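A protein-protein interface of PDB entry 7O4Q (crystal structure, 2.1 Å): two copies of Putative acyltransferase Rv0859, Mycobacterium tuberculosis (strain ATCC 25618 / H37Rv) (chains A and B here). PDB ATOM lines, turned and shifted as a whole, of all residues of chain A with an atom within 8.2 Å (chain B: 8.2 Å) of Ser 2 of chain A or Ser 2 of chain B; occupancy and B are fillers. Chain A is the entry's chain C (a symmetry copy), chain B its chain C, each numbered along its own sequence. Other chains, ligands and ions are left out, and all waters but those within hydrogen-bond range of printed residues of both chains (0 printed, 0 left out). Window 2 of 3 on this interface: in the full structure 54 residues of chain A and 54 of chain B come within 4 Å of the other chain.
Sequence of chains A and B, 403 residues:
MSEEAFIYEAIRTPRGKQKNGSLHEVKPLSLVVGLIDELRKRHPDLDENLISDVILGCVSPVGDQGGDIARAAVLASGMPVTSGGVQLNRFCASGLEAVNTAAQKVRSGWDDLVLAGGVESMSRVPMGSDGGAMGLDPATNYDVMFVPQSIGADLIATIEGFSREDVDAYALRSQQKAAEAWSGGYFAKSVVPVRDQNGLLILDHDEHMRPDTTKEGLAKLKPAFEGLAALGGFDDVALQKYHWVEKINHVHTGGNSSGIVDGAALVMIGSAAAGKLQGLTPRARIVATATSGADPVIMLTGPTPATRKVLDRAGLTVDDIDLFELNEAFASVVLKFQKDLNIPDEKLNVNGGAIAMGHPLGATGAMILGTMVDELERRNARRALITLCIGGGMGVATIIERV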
ATOM      1  N   SER A   2       7.391  -1.009   7.233  1.00  0.00           N
ATOM      2  CA  SER A   2       8.379  -1.996   6.811  1.00  0.00           C
ATOM      3  C   SER A   2       8.675  -2.988   7.933  1.00  0.00           C
ATOM      4  O   SER A   2       9.645  -3.744   7.870  1.00  0.00           O
ATOM      5  CB  SER A   2       9.669  -1.307   6.362  1.00  0.00           C
ATOM      6  OG  SER A   2      10.616  -2.252   5.897  1.00  0.00           O
ATOM      7  N   GLU A   3       7.828  -2.977   8.961  1.00  0.00           N
ATOM      8  CA  GLU A   3       7.957  -3.886  10.095  1.00  0.00           C
ATOM      9  C   GLU A   3       7.181  -5.161   9.782  1.00  0.00           C
ATOM     10  O   GLU A   3       5.948  -5.163   9.801  1.00  0.00           O
ATOM     11  CB  GLU A   3       7.441  -3.223  11.369  1.00  0.00           C
ATOM     12  CG  GLU A   3       7.660  -4.042  12.626  1.00  0.00           C
ATOM     13  CD  GLU A   3       9.118  -4.109  13.024  1.00  0.00           C
ATOM     14  OE1 GLU A   3       9.848  -3.123  12.781  1.00  0.00           O
ATOM     15  OE2 GLU A   3       9.537  -5.149  13.573  1.00  0.00           O
ATOM     16  N   GLU A   4       7.901  -6.245   9.501  1.00  0.00           N
ATOM     17  CA  GLU A   4       7.254  -7.483   9.086  1.00  0.00           C
ATOM     18  C   GLU A   4       6.397  -8.058  10.208  1.00  0.00           C
ATOM     19  O   GLU A   4       6.760  -7.997  11.386  1.00  0.00           O
ATOM     20  CB  GLU A   4       8.304  -8.506   8.650  1.00  0.00           C
ATOM     21  CG  GLU A   4       9.163  -8.064   7.473  1.00  0.00           C
ATOM     22  CD  GLU A   4       8.387  -7.989   6.167  1.00  0.00           C
ATOM     23  OE1 GLU A   4       7.337  -8.658   6.049  1.00  0.00           O
ATOM     24  OE2 GLU A   4       8.831  -7.258   5.256  1.00  0.00           O
ATOM     25  N   ALA A   5       5.249  -8.619   9.834  1.00  0.00           N
ATOM     26  CA  ALA A   5       4.346  -9.269  10.775  1.00  0.00           C
ATOM     27  C   ALA A   5       4.468 -10.781  10.638  1.00  0.00           C
ATOM     28  O   ALA A   5       4.422 -11.315   9.524  1.00  0.00           O
ATOM     29  CB  ALA A   5       2.898  -8.832  10.542  1.00  0.00           C
ATOM     30  N   PHE A   6       4.621 -11.466  11.767  1.00  0.00           N
ATOM     31  CA  PHE A   6       4.824 -12.906  11.788  1.00  0.00           C
ATOM     32  C   PHE A   6       3.723 -13.588  12.587  1.00  0.00           C
ATOM     33  O   PHE A   6       3.178 -13.020  13.537  1.00  0.00           O
ATOM     34  CB  PHE A   6       6.188 -13.266  12.386  1.00  0.00           C
ATOM     35  CG  PHE A   6       7.351 -12.757  11.588  1.00  0.00           C
ATOM     36  CD1 PHE A   6       7.854 -13.493  10.528  1.00  0.00           C
ATOM     37  CD2 PHE A   6       7.942 -11.546  11.899  1.00  0.00           C
ATOM     38  CE1 PHE A   6       8.926 -13.027   9.788  1.00  0.00           C
ATOM     39  CE2 PHE A   6       9.015 -11.072  11.164  1.00  0.00           C
ATOM     40  CZ  PHE A   6       9.508 -11.813  10.108  1.00  0.00           C
ATOM     41  N   VAL A 106       0.698  -4.411  13.180  1.00  0.00           N
ATOM     42  CA  VAL A 106       2.103  -4.707  13.447  1.00  0.00           C
ATOM     43  C   VAL A 106       3.005  -3.958  12.471  1.00  0.00           C
ATOM     44  O   VAL A 106       4.050  -3.422  12.859  1.00  0.00           O
ATOM     45  CB  VAL A 106       2.356  -6.227  13.399  1.00  0.00           C
ATOM     46  CG1 VAL A 106       3.850  -6.520  13.456  1.00  0.00           C
ATOM     47  CG2 VAL A 106       1.635  -6.924  14.544  1.00  0.00           C
ATOM     48  N   ARG A 107       2.619  -3.903  11.194  1.00  0.00           N
ATOM     49  CA  ARG A 107       3.444  -3.204  10.213  1.00  0.00           C
ATOM     50  C   ARG A 107       3.506  -1.707  10.481  1.00  0.00           C
ATOM     51  O   ARG A 107       4.509  -1.064  10.153  1.00  0.00           O
ATOM     52  CB  ARG A 107       2.923  -3.453   8.800  1.00  0.00           C
ATOM     53  CG  ARG A 107       3.193  -4.843   8.276  1.00  0.00           C
ATOM     54  CD  ARG A 107       2.758  -4.955   6.834  1.00  0.00           C
ATOM     55  NE  ARG A 107       3.609  -4.197   5.922  1.00  0.00           N
ATOM     56  CZ  ARG A 107       4.609  -4.725   5.223  1.00  0.00           C
ATOM     57  NH1 ARG A 107       4.886  -6.016   5.333  1.00  0.00           N
ATOM     58  NH2 ARG A 107       5.330  -3.963   4.414  1.00  0.00           N
ATOM     59  N   SER A 108       2.452  -1.136  11.067  1.00  0.00           N
ATOM     60  CA  SER A 108       2.436   0.298  11.326  1.00  0.00           C
ATOM     61  C   SER A 108       3.464   0.708  12.370  1.00  0.00           C
ATOM     62  O   SER A 108       3.809   1.893  12.451  1.00  0.00           O
ATOM     63  CB  SER A 108       1.044   0.735  11.781  1.00  0.00           C
ATOM     64  OG  SER A 108       0.774   0.262  13.090  1.00  0.00           O
ATOM     65  N   GLY A 109       3.963  -0.239  13.162  1.00  0.00           N
ATOM     66  CA  GLY A 109       4.883   0.067  14.235  1.00  0.00           C
ATOM     67  C   GLY A 109       4.234   0.561  15.508  1.00  0.00           C
ATOM     68  O   GLY A 109       4.948   0.841  16.478  1.00  0.00           O
ATOM     69  N   SER B   2       6.431   2.596   6.914  1.00  0.00           N
ATOM     70  CA  SER B   2       6.974   3.950   6.868  1.00  0.00           C
ATOM     71  C   SER B   2       6.184   4.824   5.897  1.00  0.00           C
ATOM     72  O   SER B   2       6.620   5.915   5.531  1.00  0.00           O
ATOM     73  CB  SER B   2       8.451   3.923   6.472  1.00  0.00           C
ATOM     74  OG  SER B   2       9.005   5.227   6.480  1.00  0.00           O
ATOM     75  N   GLU B   3       5.018   4.331   5.483  1.00  0.00           N
ATOM     76  CA  GLU B   3       4.134   5.059   4.580  1.00  0.00           C
ATOM     77  C   GLU B   3       3.196   5.924   5.416  1.00  0.00           C
ATOM     78  O   GLU B   3       2.274   5.410   6.054  1.00  0.00           O
ATOM     79  CB  GLU B   3       3.352   4.086   3.702  1.00  0.00           C
ATOM     80  CG  GLU B   3       2.506   4.754   2.636  1.00  0.00           C
ATOM     81  CD  GLU B   3       3.344   5.372   1.538  1.00  0.00           C
ATOM     82  OE1 GLU B   3       4.422   4.818   1.229  1.00  0.00           O
ATOM     83  OE2 GLU B   3       2.929   6.412   0.988  1.00  0.00           O
ATOM     84  N   GLU B   4       3.426   7.235   5.407  1.00  0.00           N
ATOM     85  CA  GLU B   4       2.654   8.134   6.256  1.00  0.00           C
ATOM     86  C   GLU B   4       1.186   8.152   5.843  1.00  0.00           C
ATOM     87  O   GLU B   4       0.854   8.099   4.655  1.00  0.00           O
ATOM     88  CB  GLU B   4       3.234   9.547   6.194  1.00  0.00           C
ATOM     89  CG  GLU B   4       4.677   9.655   6.668  1.00  0.00           C
ATOM     90  CD  GLU B   4       4.828   9.431   8.164  1.00  0.00           C
ATOM     91  OE1 GLU B   4       3.837   9.612   8.906  1.00  0.00           O
ATOM     92  OE2 GLU B   4       5.943   9.074   8.599  1.00  0.00           O
ATOM     93  N   ALA B   5       0.303   8.227   6.837  1.00  0.00           N
ATOM     94  CA  ALA B   5      -1.134   8.317   6.610  1.00  0.00           C
ATOM     95  C   ALA B   5      -1.599   9.747   6.852  1.00  0.00           C
ATOM     96  O   ALA B   5      -1.264  10.350   7.878  1.00  0.00           O
ATOM     97  CB  ALA B   5      -1.898   7.352   7.518  1.00  0.00           C
ATOM     98  N   PHE B   6      -2.371  10.284   5.912  1.00  0.00           N
ATOM     99  CA  PHE B   6      -2.831  11.662   5.969  1.00  0.00           C
ATOM    100  C   PHE B   6      -4.352  11.717   5.970  1.00  0.00           C
ATOM    101  O   PHE B   6      -5.023  10.859   5.392  1.00  0.00           O
ATOM    102  CB  PHE B   6      -2.290  12.479   4.790  1.00  0.00           C
ATOM    103  CG  PHE B   6      -0.797  12.605   4.777  1.00  0.00           C
ATOM    104  CD1 PHE B   6      -0.169  13.612   5.492  1.00  0.00           C
ATOM    105  CD2 PHE B   6      -0.022  11.721   4.049  1.00  0.00           C
ATOM    106  CE1 PHE B   6       1.209  13.732   5.483  1.00  0.00           C
ATOM    107  CE2 PHE B   6       1.358  11.834   4.036  1.00  0.00           C
ATOM    108  CZ  PHE B   6       1.974  12.840   4.753  1.00  0.00           C
ATOM    109  N   VAL B 106      -3.083   2.121   5.913  1.00  0.00           N
ATOM    110  CA  VAL B 106      -2.310   2.938   4.982  1.00  0.00           C
ATOM    111  C   VAL B 106      -0.815   2.762   5.225  1.00  0.00           C
ATOM    112  O   VAL B 106      -0.025   2.665   4.278  1.00  0.00           O
ATOM    113  CB  VAL B 106      -2.730   4.417   5.080  1.00  0.00           C
ATOM    114  CG1 VAL B 106      -1.779   5.295   4.277  1.00  0.00           C
ATOM    115  CG2 VAL B 106      -4.160   4.599   4.592  1.00  0.00           C
ATOM    116  N   ARG B 107      -0.399   2.714   6.494  1.00  0.00           N
ATOM    117  CA  ARG B 107       1.021   2.552   6.790  1.00  0.00           C
ATOM    118  C   ARG B 107       1.548   1.197   6.342  1.00  0.00           C
ATOM    119  O   ARG B 107       2.730   1.076   6.002  1.00  0.00           O
ATOM    120  CB  ARG B 107       1.283   2.739   8.281  1.00  0.00           C
ATOM    121  CG  ARG B 107       1.182   4.170   8.754  1.00  0.00           C
ATOM    122  CD  ARG B 107       1.580   4.273  10.208  1.00  0.00           C
ATOM    123  NE  ARG B 107       3.007   4.061  10.424  1.00  0.00           N
ATOM    124  CZ  ARG B 107       3.897   5.040  10.546  1.00  0.00           C
ATOM    125  NH1 ARG B 107       3.506   6.304  10.471  1.00  0.00           N
ATOM    126  NH2 ARG B 107       5.175   4.757  10.745  1.00  0.00           N
ATOM    127  N   SER B 108       0.696   0.169   6.338  1.00  0.00           N
ATOM    128  CA  SER B 108       1.143  -1.162   5.947  1.00  0.00           C
ATOM    129  C   SER B 108       1.519  -1.235   4.474  1.00  0.00           C
ATOM    130  O   SER B 108       2.224  -2.170   4.073  1.00  0.00           O
ATOM    131  CB  SER B 108       0.056  -2.192   6.249  1.00  0.00           C
ATOM    132  OG  SER B 108      -1.034  -2.045   5.355  1.00  0.00           O
ATOM    133  N   GLY B 109       1.074  -0.276   3.666  1.00  0.00           N
ATOM    134  CA  GLY B 109       1.310  -0.305   2.240  1.00  0.00           C
ATOM    135  C   GLY B 109       0.362  -1.182   1.455  1.00  0.00           C
ATOM    136  O   GLY B 109       0.490  -1.260   0.228  1.00  0.00           O
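Of the printed residues of chain B, Ser 2 of chain A touches Ser 2.
Of the printed residues of chain B, Arg 107 of chain A touches Ser 108.
Of chain A, only Ser 2 comes within 4 Å of Ser 2 of chain B.
Glu 3 of chain B touches none of the printed residues of chain A.
Printed residues of chain A within 4 Å of Arg 107 of chain B: Ser 108.
Of the printed residues of chain A, Ser 108 of chain B touches Arg 107.
Ser 2 of chain A touches its own counterpart, Ser 2 of chain B.
Arg 107 of chain A touches Ser 108 of chain B, and with the chains exchanged Ser 108 of chain A touches Arg 107 of chain B.
Of the 3 pairs that touch across the chains among the printed residues, 3 have their exchanged pair printed and touching as well.
O of Ser 108 of chain A lies within hydrogen-bond range of NE of Arg 107 of chain B, at 3.1 Å.
NE of Arg 107 of chain A sits at hydrogen-bond distance from O of Ser 108 of chain B, 3.1 Å away.
Of the 9 printed residues of chain A, 3 touch a printed residue of chain B.
Among the printed residues, 3 pairs touch across the chains.
Among the printed residues, no Asp or Glu carboxylate lies within 4 Å of a Lys or Arg side-chain nitrogen of the other chain.
Among the printed residues, pairs that only touch across the chains: Ser 2 of chain A with Ser 2 of chain B.
The side-chain carboxylate (OE1) of Glu 4 of chain B lies within salt-bridge range of the guanidinium group (NH1) of Arg 107 of chain B, 3.7 Å away.
The side-chain carboxylate of Glu 4 of chain A lies within salt-bridge range of the guanidinium group of Arg 107 of chain A, at 3.7 Å.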
